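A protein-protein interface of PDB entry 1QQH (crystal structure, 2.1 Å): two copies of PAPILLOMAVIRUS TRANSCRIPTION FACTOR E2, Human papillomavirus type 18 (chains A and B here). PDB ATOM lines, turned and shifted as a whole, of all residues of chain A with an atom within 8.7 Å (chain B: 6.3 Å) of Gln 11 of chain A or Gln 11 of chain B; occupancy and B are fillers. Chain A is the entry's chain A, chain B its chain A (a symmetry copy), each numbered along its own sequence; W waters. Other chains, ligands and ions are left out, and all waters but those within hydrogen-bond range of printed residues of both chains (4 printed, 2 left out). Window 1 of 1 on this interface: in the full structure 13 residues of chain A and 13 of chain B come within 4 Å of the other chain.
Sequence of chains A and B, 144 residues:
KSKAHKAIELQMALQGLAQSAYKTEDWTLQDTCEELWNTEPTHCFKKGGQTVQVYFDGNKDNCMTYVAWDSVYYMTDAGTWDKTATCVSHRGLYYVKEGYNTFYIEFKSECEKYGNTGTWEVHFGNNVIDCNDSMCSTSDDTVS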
ATOM      1  N   LYS A   3       0.543 -35.352 -22.656  1.00  0.00           N
ATOM      2  CA  LYS A   3       0.357 -34.227 -21.750  1.00  0.00           C
ATOM      3  C   LYS A   3       1.562 -34.103 -20.826  1.00  0.00           C
ATOM      4  O   LYS A   3       1.924 -33.003 -20.406  1.00  0.00           O
ATOM      5  CB  LYS A   3      -0.920 -34.427 -20.927  1.00  0.00           C
ATOM      6  CG  LYS A   3      -1.305 -33.237 -20.064  1.00  0.00           C
ATOM      7  CD  LYS A   3      -2.627 -33.484 -19.357  1.00  0.00           C
ATOM      8  CE  LYS A   3      -3.056 -32.271 -18.550  1.00  0.00           C
ATOM      9  NZ  LYS A   3      -4.372 -32.482 -17.887  1.00  0.00           N
ATOM     10  N   ALA A   4       2.179 -35.239 -20.514  1.00  0.00           N
ATOM     11  CA  ALA A   4       3.353 -35.257 -19.650  1.00  0.00           C
ATOM     12  C   ALA A   4       4.397 -34.300 -20.215  1.00  0.00           C
ATOM     13  O   ALA A   4       5.115 -33.634 -19.469  1.00  0.00           O
ATOM     14  CB  ALA A   4       3.919 -36.666 -19.572  1.00  0.00           C
ATOM     15  N   HIS A   5       4.467 -34.238 -21.542  1.00  0.00           N
ATOM     16  CA  HIS A   5       5.404 -33.358 -22.228  1.00  0.00           C
ATOM     17  C   HIS A   5       4.928 -31.910 -22.131  1.00  0.00           C
ATOM     18  O   HIS A   5       5.728 -30.986 -21.960  1.00  0.00           O
ATOM     19  CB  HIS A   5       5.528 -33.770 -23.700  1.00  0.00           C
ATOM     20  CG  HIS A   5       6.273 -32.781 -24.545  1.00  0.00           C
ATOM     21  ND1 HIS A   5       7.533 -32.326 -24.223  1.00  0.00           N
ATOM     22  CD2 HIS A   5       5.932 -32.164 -25.701  1.00  0.00           C
ATOM     23  CE1 HIS A   5       7.937 -31.470 -25.145  1.00  0.00           C
ATOM     24  NE2 HIS A   5       6.986 -31.354 -26.053  1.00  0.00           N
ATOM     25  N   LYS A   6       3.616 -31.721 -22.244  1.00  0.00           N
ATOM     26  CA  LYS A   6       3.029 -30.393 -22.164  1.00  0.00           C
ATOM     27  C   LYS A   6       3.451 -29.688 -20.882  1.00  0.00           C
ATOM     28  O   LYS A   6       3.973 -28.576 -20.924  1.00  0.00           O
ATOM     29  CB  LYS A   6       1.503 -30.487 -22.242  1.00  0.00           C
ATOM     30  CG  LYS A   6       0.975 -30.735 -23.651  1.00  0.00           C
ATOM     31  CD  LYS A   6       1.211 -29.523 -24.547  1.00  0.00           C
ATOM     32  CE  LYS A   6       0.936 -29.830 -26.012  1.00  0.00           C
ATOM     33  NZ  LYS A   6       1.916 -30.810 -26.568  1.00  0.00           N
ATOM     34  N   ALA A   7       3.236 -30.340 -19.744  1.00  0.00           N
ATOM     35  CA  ALA A   7       3.604 -29.763 -18.454  1.00  0.00           C
ATOM     36  C   ALA A   7       5.054 -29.283 -18.451  1.00  0.00           C
ATOM     37  O   ALA A   7       5.385 -28.280 -17.817  1.00  0.00           O
ATOM     38  CB  ALA A   7       3.393 -30.788 -17.343  1.00  0.00           C
ATOM     39  N   ILE A   8       5.909 -30.002 -19.172  1.00  0.00           N
ATOM     40  CA  ILE A   8       7.330 -29.676 -19.251  1.00  0.00           C
ATOM     41  C   ILE A   8       7.583 -28.391 -20.039  1.00  0.00           C
ATOM     42  O   ILE A   8       8.388 -27.546 -19.637  1.00  0.00           O
ATOM     43  CB  ILE A   8       8.124 -30.820 -19.923  1.00  0.00           C
ATOM     44  CG1 ILE A   8       7.684 -32.173 -19.354  1.00  0.00           C
ATOM     45  CG2 ILE A   8       9.616 -30.618 -19.699  1.00  0.00           C
ATOM     46  CD1 ILE A   8       7.923 -32.338 -17.861  1.00  0.00           C
ATOM     47  N   GLU A   9       6.897 -28.254 -21.167  1.00  0.00           N
ATOM     48  CA  GLU A   9       7.039 -27.075 -22.013  1.00  0.00           C
ATOM     49  C   GLU A   9       6.585 -25.845 -21.234  1.00  0.00           C
ATOM     50  O   GLU A   9       7.267 -24.819 -21.199  1.00  0.00           O
ATOM     51  CB  GLU A   9       6.193 -27.248 -23.278  1.00  0.00           C
ATOM     52  CG  GLU A   9       6.387 -26.170 -24.329  1.00  0.00           C
ATOM     53  CD  GLU A   9       5.754 -26.539 -25.663  1.00  0.00           C
ATOM     54  OE1 GLU A   9       5.896 -25.755 -26.626  1.00  0.00           O
ATOM     55  OE2 GLU A   9       5.114 -27.613 -25.750  1.00  0.00           O
ATOM     56  N   LEU A  10       5.425 -25.967 -20.598  1.00  0.00           N
ATOM     57  CA  LEU A  10       4.863 -24.885 -19.808  1.00  0.00           C
ATOM     58  C   LEU A  10       5.829 -24.467 -18.702  1.00  0.00           C
ATOM     59  O   LEU A  10       6.057 -23.280 -18.474  1.00  0.00           O
ATOM     60  CB  LEU A  10       3.529 -25.327 -19.202  1.00  0.00           C
ATOM     61  CG  LEU A  10       2.841 -24.345 -18.258  1.00  0.00           C
ATOM     62  CD1 LEU A  10       2.628 -23.025 -18.963  1.00  0.00           C
ATOM     63  CD2 LEU A  10       1.518 -24.928 -17.780  1.00  0.00           C
ATOM     64  N   GLN A  11       6.403 -25.452 -18.022  1.00  0.00           N
ATOM     65  CA  GLN A  11       7.335 -25.172 -16.940  1.00  0.00           C
ATOM     66  C   GLN A  11       8.542 -24.374 -17.423  1.00  0.00           C
ATOM     67  O   GLN A  11       8.948 -23.403 -16.787  1.00  0.00           O
ATOM     68  CB  GLN A  11       7.813 -26.467 -16.306  1.00  0.00           C
ATOM     69  CG  GLN A  11       8.155 -26.292 -14.850  1.00  0.00           C
ATOM     70  CD  GLN A  11       6.918 -26.025 -14.023  1.00  0.00           C
ATOM     71  OE1 GLN A  11       6.038 -26.882 -13.913  1.00  0.00           O
ATOM     72  NE2 GLN A  11       6.836 -24.830 -13.443  1.00  0.00           N
ATOM     73  N   MET A  12       9.124 -24.793 -18.541  1.00  0.00           N
ATOM     74  CA  MET A  12      10.270 -24.080 -19.078  1.00  0.00           C
ATOM     75  C   MET A  12       9.869 -22.657 -19.442  1.00  0.00           C
ATOM     76  O   MET A  12      10.603 -21.706 -19.159  1.00  0.00           O
ATOM     77  CB  MET A  12      10.836 -24.803 -20.300  1.00  0.00           C
ATOM     78  CG  MET A  12      11.610 -26.073 -19.946  1.00  0.00           C
ATOM     79  SD  MET A  12      12.820 -25.810 -18.592  1.00  0.00           S
ATOM     80  CE  MET A  12      14.096 -24.812 -19.450  1.00  0.00           C
ATOM     81  N   ALA A  13       8.697 -22.510 -20.054  1.00  0.00           N
ATOM     82  CA  ALA A  13       8.207 -21.189 -20.434  1.00  0.00           C
ATOM     83  C   ALA A  13       8.109 -20.311 -19.190  1.00  0.00           C
ATOM     84  O   ALA A  13       8.555 -19.160 -19.193  1.00  0.00           O
ATOM     85  CB  ALA A  13       6.844 -21.306 -21.100  1.00  0.00           C
ATOM     86  N   LEU A  14       7.527 -20.860 -18.128  1.00  0.00           N
ATOM     87  CA  LEU A  14       7.379 -20.125 -16.879  1.00  0.00           C
ATOM     88  C   LEU A  14       8.742 -19.777 -16.271  1.00  0.00           C
ATOM     89  O   LEU A  14       8.892 -18.737 -15.633  1.00  0.00           O
ATOM     90  CB  LEU A  14       6.533 -20.930 -15.880  1.00  0.00           C
ATOM     91  CG  LEU A  14       5.032 -21.052 -16.184  1.00  0.00           C
ATOM     92  CD1 LEU A  14       4.395 -22.045 -15.236  1.00  0.00           C
ATOM     93  CD2 LEU A  14       4.363 -19.696 -16.062  1.00  0.00           C
ATOM     94  N   GLN A  15       9.735 -20.643 -16.463  1.00  0.00           N
ATOM     95  CA  GLN A  15      11.073 -20.356 -15.947  1.00  0.00           C
ATOM     96  C   GLN A  15      11.595 -19.126 -16.685  1.00  0.00           C
ATOM     97  O   GLN A  15      12.174 -18.227 -16.080  1.00  0.00           O
ATOM     98  CB  GLN A  15      12.014 -21.548 -16.169  1.00  0.00           C
ATOM     99  CG  GLN A  15      12.312 -22.337 -14.896  1.00  0.00           C
ATOM    100  CD  GLN A  15      12.102 -23.839 -15.062  1.00  0.00           C
ATOM    101  OE1 GLN A  15      12.701 -24.474 -15.940  1.00  0.00           O
ATOM    102  NE2 GLN A  15      11.251 -24.415 -14.213  1.00  0.00           N
ATOM    103  N   GLY A  16      11.369 -19.080 -17.996  1.00  0.00           N
ATOM    104  CA  GLY A  16      11.819 -17.936 -18.770  1.00  0.00           C
ATOM    105  C   GLY A  16      11.037 -16.688 -18.405  1.00  0.00           C
ATOM    106  O   GLY A  16      11.599 -15.601 -18.234  1.00  0.00           O
ATOM    107  N   LEU A  17       9.723 -16.843 -18.280  1.00  0.00           N
ATOM    108  CA  LEU A  17       8.858 -15.727 -17.931  1.00  0.00           C
ATOM    109  C   LEU A  17       9.275 -15.160 -16.577  1.00  0.00           C
ATOM    110  O   LEU A  17       9.277 -13.947 -16.372  1.00  0.00           O
ATOM    111  CB  LEU A  17       7.396 -16.196 -17.879  1.00  0.00           C
ATOM    112  CG  LEU A  17       6.342 -15.114 -17.611  1.00  0.00           C
ATOM    113  CD1 LEU A  17       6.347 -14.095 -18.753  1.00  0.00           C
ATOM    114  CD2 LEU A  17       4.956 -15.752 -17.471  1.00  0.00           C
ATOM    115  N   ALA A  18       9.640 -16.050 -15.659  1.00  0.00           N
ATOM    116  CA  ALA A  18      10.046 -15.651 -14.315  1.00  0.00           C
ATOM    117  C   ALA A  18      11.298 -14.773 -14.309  1.00  0.00           C
ATOM    118  O   ALA A  18      11.536 -14.015 -13.365  1.00  0.00           O
ATOM    119  CB  ALA A  18      10.269 -16.885 -13.460  1.00  0.00           C
ATOM    120  N   LEU A  29      -2.870 -17.787 -10.828  1.00  0.00           N
ATOM    121  CA  LEU A  29      -2.667 -19.203 -11.085  1.00  0.00           C
ATOM    122  C   LEU A  29      -3.313 -19.517 -12.426  1.00  0.00           C
ATOM    123  O   LEU A  29      -2.786 -20.291 -13.217  1.00  0.00           O
ATOM    124  CB  LEU A  29      -3.306 -20.027  -9.969  1.00  0.00           C
ATOM    125  CG  LEU A  29      -2.604 -19.796  -8.630  1.00  0.00           C
ATOM    126  CD1 LEU A  29      -3.401 -20.391  -7.476  1.00  0.00           C
ATOM    127  CD2 LEU A  29      -1.211 -20.413  -8.716  1.00  0.00           C
ATOM    128  N   THR A  32      -1.267 -18.768 -15.550  1.00  0.00           N
ATOM    129  CA  THR A  32      -0.179 -19.702 -15.801  1.00  0.00           C
ATOM    130  C   THR A  32      -0.558 -21.168 -15.923  1.00  0.00           C
ATOM    131  O   THR A  32       0.326 -22.014 -16.036  1.00  0.00           O
ATOM    132  CB  THR A  32       0.894 -19.589 -14.692  1.00  0.00           C
ATOM    133  OG1 THR A  32       0.305 -19.895 -13.421  1.00  0.00           O
ATOM    134  CG2 THR A  32       1.462 -18.179 -14.636  1.00  0.00           C
ATOM    135  N   CYS A  33      -1.851 -21.483 -15.922  1.00  0.00           N
ATOM    136  CA  CYS A  33      -2.254 -22.886 -15.996  1.00  0.00           C
ATOM    137  C   CYS A  33      -2.134 -23.505 -17.385  1.00  0.00           C
ATOM    138  O   CYS A  33      -2.035 -22.804 -18.389  1.00  0.00           O
ATOM    139  CB  CYS A  33      -3.682 -23.062 -15.467  1.00  0.00           C
ATOM    140  SG  CYS A  33      -4.984 -22.515 -16.589  1.00  0.00           S
ATOM    141  N   GLU A  34      -2.141 -24.836 -17.421  1.00  0.00           N
ATOM    142  CA  GLU A  34      -2.022 -25.597 -18.660  1.00  0.00           C
ATOM    143  C   GLU A  34      -3.170 -25.356 -19.627  1.00  0.00           C
ATOM    144  O   GLU A  34      -2.949 -25.193 -20.828  1.00  0.00           O
ATOM    145  CB  GLU A  34      -1.935 -27.096 -18.358  1.00  0.00           C
ATOM    146  CG  GLU A  34      -0.554 -27.582 -17.940  1.00  0.00           C
ATOM    147  CD  GLU A  34      -0.555 -29.030 -17.436  1.00  0.00           C
ATOM    148  OE1 GLU A  34       0.548 -29.583 -17.210  1.00  0.00           O
ATOM    149  OE2 GLU A  34      -1.652 -29.612 -17.263  1.00  0.00           O
ATOM    150  N   GLU A  35      -4.394 -25.341 -19.107  1.00  0.00           N
ATOM    151  CA  GLU A  35      -5.565 -25.136 -19.954  1.00  0.00           C
ATOM    152  C   GLU A  35      -5.426 -23.897 -20.829  1.00  0.00           C
ATOM    153  O   GLU A  35      -5.656 -23.948 -22.037  1.00  0.00           O
ATOM    154  CB  GLU A  35      -6.834 -25.015 -19.109  1.00  0.00           C
ATOM    155  CG  GLU A  35      -7.406 -26.331 -18.615  1.00  0.00           C
ATOM    156  CD  GLU A  35      -7.757 -27.287 -19.748  1.00  0.00           C
ATOM    157  OE1 GLU A  35      -8.190 -26.824 -20.835  1.00  0.00           O
ATOM    158  OE2 GLU A  35      -7.611 -28.511 -19.541  1.00  0.00           O
ATOM    159  N   TRP A  37      -2.595 -22.211 -21.343  1.00  0.00           N
ATOM    160  CA  TRP A  37      -1.359 -22.354 -22.091  1.00  0.00           C
ATOM    161  C   TRP A  37      -1.648 -23.013 -23.433  1.00  0.00           C
ATOM    162  O   TRP A  37      -1.100 -22.614 -24.457  1.00  0.00           O
ATOM    163  CB  TRP A  37      -0.370 -23.194 -21.282  1.00  0.00           C
ATOM    164  CG  TRP A  37       0.899 -23.553 -22.005  1.00  0.00           C
ATOM    165  CD1 TRP A  37       1.286 -24.801 -22.419  1.00  0.00           C
ATOM    166  CD2 TRP A  37       1.940 -22.658 -22.412  1.00  0.00           C
ATOM    167  NE1 TRP A  37       2.502 -24.736 -23.056  1.00  0.00           N
ATOM    168  CE2 TRP A  37       2.926 -23.433 -23.068  1.00  0.00           C
ATOM    169  CE3 TRP A  37       2.136 -21.275 -22.289  1.00  0.00           C
ATOM    170  CZ2 TRP A  37       4.092 -22.868 -23.599  1.00  0.00           C
ATOM    171  CZ3 TRP A  37       3.292 -20.714 -22.818  1.00  0.00           C
ATOM    172  CH2 TRP A  37       4.257 -21.514 -23.466  1.00  0.00           C
ATOM    173  N   PHE A  45       1.596 -16.484 -23.361  1.00  0.00           N
ATOM    174  CA  PHE A  45       0.864 -16.229 -22.134  1.00  0.00           C
ATOM    175  C   PHE A  45      -0.024 -15.060 -22.538  1.00  0.00           C
ATOM    176  O   PHE A  45       0.312 -14.297 -23.441  1.00  0.00           O
ATOM    177  CB  PHE A  45       1.798 -15.851 -20.969  1.00  0.00           C
ATOM    178  CG  PHE A  45       2.591 -17.018 -20.432  1.00  0.00           C
ATOM    179  CD1 PHE A  45       3.955 -17.145 -20.697  1.00  0.00           C
ATOM    180  CD2 PHE A  45       1.958 -18.029 -19.721  1.00  0.00           C
ATOM    181  CE1 PHE A  45       4.669 -18.269 -20.265  1.00  0.00           C
ATOM    182  CE2 PHE A  45       2.662 -19.148 -19.287  1.00  0.00           C
ATOM    183  CZ  PHE A  45       4.018 -19.268 -19.563  1.00  0.00           C
ATOM    184  N   TRP A  81      11.160 -12.730 -23.955  1.00  0.00           N
ATOM    185  CA  TRP A  81       9.720 -12.510 -23.916  1.00  0.00           C
ATOM    186  C   TRP A  81       9.303 -11.085 -24.235  1.00  0.00           C
ATOM    187  O   TRP A  81       9.773 -10.134 -23.614  1.00  0.00           O
ATOM    188  CB  TRP A  81       9.154 -12.901 -22.541  1.00  0.00           C
ATOM    189  CG  TRP A  81       9.205 -14.362 -22.284  1.00  0.00           C
ATOM    190  CD1 TRP A  81      10.233 -15.059 -21.727  1.00  0.00           C
ATOM    191  CD2 TRP A  81       8.219 -15.330 -22.661  1.00  0.00           C
ATOM    192  NE1 TRP A  81       9.954 -16.403 -21.739  1.00  0.00           N
ATOM    193  CE2 TRP A  81       8.724 -16.598 -22.307  1.00  0.00           C
ATOM    194  CE3 TRP A  81       6.957 -15.247 -23.269  1.00  0.00           C
ATOM    195  CZ2 TRP A  81       8.015 -17.781 -22.542  1.00  0.00           C
ATOM    196  CZ3 TRP A  81       6.253 -16.418 -23.505  1.00  0.00           C
ATOM    197  CH2 TRP A  81       6.786 -17.670 -23.140  1.00  0.00           C
ATOM    198  N   LYS B   6       9.138 -34.315 -11.735  1.00  0.00           N
ATOM    199  CA  LYS B   6       8.955 -33.209 -10.810  1.00  0.00           C
ATOM    200  C   LYS B   6       7.984 -32.181 -11.376  1.00  0.00           C
ATOM    201  O   LYS B   6       7.000 -31.830 -10.729  1.00  0.00           O
ATOM    202  CB  LYS B   6      10.303 -32.555 -10.500  1.00  0.00           C
ATOM    203  CG  LYS B   6      11.162 -33.350  -9.522  1.00  0.00           C
ATOM    204  CD  LYS B   6      10.543 -33.355  -8.127  1.00  0.00           C
ATOM    205  CE  LYS B   6      11.229 -34.346  -7.199  1.00  0.00           C
ATOM    206  NZ  LYS B   6      11.005 -35.758  -7.631  1.00  0.00           N
ATOM    207  N   ALA B   7       8.257 -31.709 -12.587  1.00  0.00           N
ATOM    208  CA  ALA B   7       7.393 -30.722 -13.232  1.00  0.00           C
ATOM    209  C   ALA B   7       5.932 -31.165 -13.220  1.00  0.00           C
ATOM    210  O   ALA B   7       5.024 -30.343 -13.100  1.00  0.00           O
ATOM    211  CB  ALA B   7       7.853 -30.482 -14.667  1.00  0.00           C
ATOM    212  N   ILE B   8       5.718 -32.474 -13.336  1.00  0.00           N
ATOM    213  CA  ILE B   8       4.374 -33.046 -13.359  1.00  0.00           C
ATOM    214  C   ILE B   8       3.684 -32.946 -11.998  1.00  0.00           C
ATOM    215  O   ILE B   8       2.503 -32.600 -11.909  1.00  0.00           O
ATOM    216  CB  ILE B   8       4.413 -34.534 -13.774  1.00  0.00           C
ATOM    217  CG1 ILE B   8       5.341 -34.721 -14.980  1.00  0.00           C
ATOM    218  CG2 ILE B   8       3.010 -35.015 -14.113  1.00  0.00           C
ATOM    219  CD1 ILE B   8       4.915 -33.964 -16.228  1.00  0.00           C
ATOM    220  N   GLU B   9       4.426 -33.259 -10.943  1.00  0.00           N
ATOM    221  CA  GLU B   9       3.893 -33.203  -9.587  1.00  0.00           C
ATOM    222  C   GLU B   9       3.504 -31.764  -9.264  1.00  0.00           C
ATOM    223  O   GLU B   9       2.410 -31.492  -8.762  1.00  0.00           O
ATOM    224  CB  GLU B   9       4.952 -33.703  -8.600  1.00  0.00           C
ATOM    225  CG  GLU B   9       4.468 -33.864  -7.171  1.00  0.00           C
ATOM    226  CD  GLU B   9       5.459 -34.628  -6.305  1.00  0.00           C
ATOM    227  OE1 GLU B   9       5.148 -34.875  -5.120  1.00  0.00           O
ATOM    228  OE2 GLU B   9       6.551 -34.984  -6.808  1.00  0.00           O
ATOM    229  N   LEU B  10       4.410 -30.843  -9.569  1.00  0.00           N
ATOM    230  CA  LEU B  10       4.183 -29.428  -9.328  1.00  0.00           C
ATOM    231  C   LEU B  10       2.933 -28.950 -10.064  1.00  0.00           C
ATOM    232  O   LEU B  10       2.104 -28.235  -9.506  1.00  0.00           O
ATOM    233  CB  LEU B  10       5.402 -28.625  -9.785  1.00  0.00           C
ATOM    234  CG  LEU B  10       5.299 -27.105  -9.696  1.00  0.00           C
ATOM    235  CD1 LEU B  10       4.967 -26.699  -8.278  1.00  0.00           C
ATOM    236  CD2 LEU B  10       6.606 -26.469 -10.152  1.00  0.00           C
ATOM    237  N   GLN B  11       2.800 -29.360 -11.321  1.00  0.00           N
ATOM    238  CA  GLN B  11       1.653 -28.959 -12.121  1.00  0.00           C
ATOM    239  C   GLN B  11       0.338 -29.416 -11.497  1.00  0.00           C
ATOM    240  O   GLN B  11      -0.618 -28.647 -11.415  1.00  0.00           O
ATOM    241  CB  GLN B  11       1.764 -29.529 -13.526  1.00  0.00           C
ATOM    242  CG  GLN B  11       1.091 -28.652 -14.546  1.00  0.00           C
ATOM    243  CD  GLN B  11       1.829 -27.344 -14.723  1.00  0.00           C
ATOM    244  OE1 GLN B  11       2.975 -27.328 -15.181  1.00  0.00           O
ATOM    245  NE2 GLN B  11       1.184 -26.241 -14.354  1.00  0.00           N
ATOM    246  N   MET B  12       0.286 -30.674 -11.072  1.00  0.00           N
ATOM    247  CA  MET B  12      -0.923 -31.184 -10.451  1.00  0.00           C
ATOM    248  C   MET B  12      -1.220 -30.404  -9.177  1.00  0.00           C
ATOM    249  O   MET B  12      -2.369 -30.040  -8.917  1.00  0.00           O
ATOM    250  CB  MET B  12      -0.790 -32.676 -10.145  1.00  0.00           C
ATOM    251  CG  MET B  12      -0.882 -33.560 -11.388  1.00  0.00           C
ATOM    252  SD  MET B  12      -2.311 -33.130 -12.455  1.00  0.00           S
ATOM    253  CE  MET B  12      -3.706 -33.751 -11.442  1.00  0.00           C
ATOM    254  N   ALA B  13      -0.179 -30.134  -8.393  1.00  0.00           N
ATOM    255  CA  ALA B  13      -0.345 -29.378  -7.155  1.00  0.00           C
ATOM    256  C   ALA B  13      -0.956 -28.018  -7.474  1.00  0.00           C
ATOM    257  O   ALA B  13      -1.904 -27.581  -6.815  1.00  0.00           O
ATOM    258  CB  ALA B  13       0.999 -29.201  -6.464  1.00  0.00           C
ATOM    259  N   LEU B  14      -0.410 -27.352  -8.489  1.00  0.00           N
ATOM    260  CA  LEU B  14      -0.909 -26.045  -8.894  1.00  0.00           C
ATOM    261  C   LEU B  14      -2.356 -26.129  -9.392  1.00  0.00           C
ATOM    262  O   LEU B  14      -3.131 -25.191  -9.214  1.00  0.00           O
ATOM    263  CB  LEU B  14      -0.001 -25.437  -9.974  1.00  0.00           C
ATOM    264  CG  LEU B  14       1.388 -24.957  -9.522  1.00  0.00           C
ATOM    265  CD1 LEU B  14       2.224 -24.594 -10.730  1.00  0.00           C
ATOM    266  CD2 LEU B  14       1.251 -23.765  -8.592  1.00  0.00           C
ATOM    267  N   GLN B  15      -2.722 -27.244 -10.019  1.00  0.00           N
ATOM    268  CA  GLN B  15      -4.097 -27.411 -10.485  1.00  0.00           C
ATOM    269  C   GLN B  15      -4.998 -27.444  -9.253  1.00  0.00           C
ATOM    270  O   GLN B  15      -6.058 -26.823  -9.230  1.00  0.00           O
ATOM    271  CB  GLN B  15      -4.251 -28.707 -11.291  1.00  0.00           C
ATOM    272  CG  GLN B  15      -4.372 -28.481 -12.797  1.00  0.00           C
ATOM    273  CD  GLN B  15      -3.413 -29.346 -13.608  1.00  0.00           C
ATOM    274  OE1 GLN B  15      -3.421 -30.580 -13.502  1.00  0.00           O
ATOM    275  NE2 GLN B  15      -2.583 -28.701 -14.429  1.00  0.00           N
ATOM    276  N   GLY B  16      -4.561 -28.157  -8.217  1.00  0.00           N
ATOM    277  CA  GLY B  16      -5.351 -28.228  -7.000  1.00  0.00           C
ATOM    278  C   GLY B  16      -5.388 -26.885  -6.294  1.00  0.00           C
ATOM    279  O   GLY B  16      -6.437 -26.430  -5.829  1.00  0.00           O
ATOM    280  N   THR B  32       5.427 -20.098  -7.206  1.00  0.00           N
ATOM    281  CA  THR B  32       5.028 -21.339  -7.853  1.00  0.00           C
ATOM    282  C   THR B  32       6.101 -22.070  -8.638  1.00  0.00           C
ATOM    283  O   THR B  32       5.801 -23.070  -9.288  1.00  0.00           O
ATOM    284  CB  THR B  32       3.838 -21.087  -8.811  1.00  0.00           C
ATOM    285  OG1 THR B  32       4.227 -20.143  -9.818  1.00  0.00           O
ATOM    286  CG2 THR B  32       2.647 -20.524  -8.052  1.00  0.00           C
ATOM    287  N   CYS B  33       7.348 -21.607  -8.579  1.00  0.00           N
ATOM    288  CA  CYS B  33       8.401 -22.261  -9.353  1.00  0.00           C
ATOM    289  C   CYS B  33       8.893 -23.578  -8.765  1.00  0.00           C
ATOM    290  O   CYS B  33       8.667 -23.878  -7.595  1.00  0.00           O
ATOM    291  CB  CYS B  33       9.583 -21.306  -9.561  1.00  0.00           C
ATOM    292  SG  CYS B  33      10.638 -21.073  -8.118  1.00  0.00           S
ATOM    293  N   GLU B  34       9.569 -24.362  -9.602  1.00  0.00           N
ATOM    294  CA  GLU B  34      10.102 -25.664  -9.215  1.00  0.00           C
ATOM    295  C   GLU B  34      11.149 -25.583  -8.116  1.00  0.00           C
ATOM    296  O   GLU B  34      11.128 -26.380  -7.177  1.00  0.00           O
ATOM    297  CB  GLU B  34      10.713 -26.371 -10.429  1.00  0.00           C
ATOM    298  CG  GLU B  34       9.706 -27.065 -11.335  1.00  0.00           C
ATOM    299  CD  GLU B  34      10.324 -27.569 -12.644  1.00  0.00           C
ATOM    300  OE1 GLU B  34       9.623 -28.288 -13.396  1.00  0.00           O
ATOM    301  OE2 GLU B  34      11.502 -27.244 -12.924  1.00  0.00           O
HETATM  302  O   HOH W   1       2.513 -20.811 -11.947  1.00  0.00           O
HETATM  303  O   HOH W   2       3.710 -24.593 -13.511  1.00  0.00           O
HETATM  304  O   HOH W   3       0.999 -23.108 -13.774  1.00  0.00           O
HETATM  305  O   HOH W   4       5.314 -22.562 -11.792  1.00  0.00           O
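NE2 of Gln 15 of chain A is in hydrogen-bond range of OE2 of Glu 34 of chain B, at 3.1 Å.
The side-chain carboxylate of Glu 34 of chain A sits at hydrogen-bond distance from the side-chain amide nitrogen of Gln 15 of chain B (3.1 Å).
OE1 of Gln 11 of chain A lies close to OE1 of Gln 11 of chain B (3.3 Å).
SD of Met 12 of chain A sits close to OE1 of Gln 15 of chain A, 3.0 Å away.
The side-chain sulfur (SD) of Met 12 of chain B sits close to the side-chain amide oxygen (OE1) of Gln 15 of chain B (3.0 Å).
OG1 of Thr 32 of chain A is in hydrogen-bond range of O of Leu 29 of chain A, 3.1 Å away.
Among the printed residues, pairs that only touch across the chains: Ala 4 of chain A with Ile 8 of chain B, Ala 7 of chain A with Ile 8 of chain B, Ala 7 of chain A with Gln 11 of chain B, Ile 8 of chain A with Ala 7 of chain B, Ile 8 of chain A with Ile 8 of chain B, Leu 10 of chain A with Gln 11 of chain B, Gln 11 of chain A with Ala 7 of chain B, Gln 11 of chain A with Leu 10 of chain B, Gln 11 of chain A with Glu 34 of chain B, Leu 29 of chain A with Thr 32 of chain B and Glu 34 of chain A with Gln 11 of chain B.
Of the printed residues of chain A, Gln 11 of chain B touches Ala 7, Leu 10, Gln 11 and Glu 34.
Of chain A, only Gln 11 (3.7 Å) comes within 4 Å of Leu 10 of chain B.
Of the printed residues of chain B, Leu 10 of chain A touches Gln 11 (3.7 Å).
Of the printed residues of chain A, Gln 15 of chain B touches Glu 34.
Of the printed residues of chain B, Glu 34 of chain A touches Gln 11 (2.9 Å) and Gln 15 (3.1 Å).
Leu 14 of chain A touches none of the printed residues of chain B.
The nearest residue of chain A that does not touch Gln 11 of chain B is Thr 32 of chain A (4.6 Å).
Of the 14 printed residues of chain B, 7 touch a printed residue of chain A.
Hydrophobic or aromatic side chains of chain B that line the printed part of chain A: Ala 7, Ile 8 and Leu 10.
Of the 24 printed residues of chain A, 8 touch a printed residue of chain B.
Printed residues of chain A that touch a printed residue of chain B: Ala 4, Ala 7, Ile 8, Leu 10, Gln 11, Gln 15, Leu 29 and Glu 34.
Hydrophobic or aromatic side chains of chain A that line the printed part of chain B: Ala 7, Ile 8, Leu 10 and Leu 29.
Among the printed residues, 14 pairs touch across the chains.
Leu 10 of chain A touches Gln 11 of chain B, and with the chains exchanged Gln 11 of chain A touches Leu 10 of chain B.
Gln 11 of chain A touches Glu 34 of chain B, and with the chains exchanged Glu 34 of chain A touches Gln 11 of chain B.
Gln 15 of chain A touches Glu 34 of chain B, and with the chains exchanged Glu 34 of chain A touches Gln 15 of chain B.
Water W3 bridges the backbone carbonyl oxygen of Thr 32 of chain A (2.6 Å) and the side-chain amide nitrogen of Gln 11 of chain B (3.2 Å).
Water W2 bridges the side-chain amide nitrogen (NE2) of Gln 11 of chain B (3.1 Å) and the side-chain amide nitrogen (NE2) of Gln 11 of chain A (3.1 Å).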
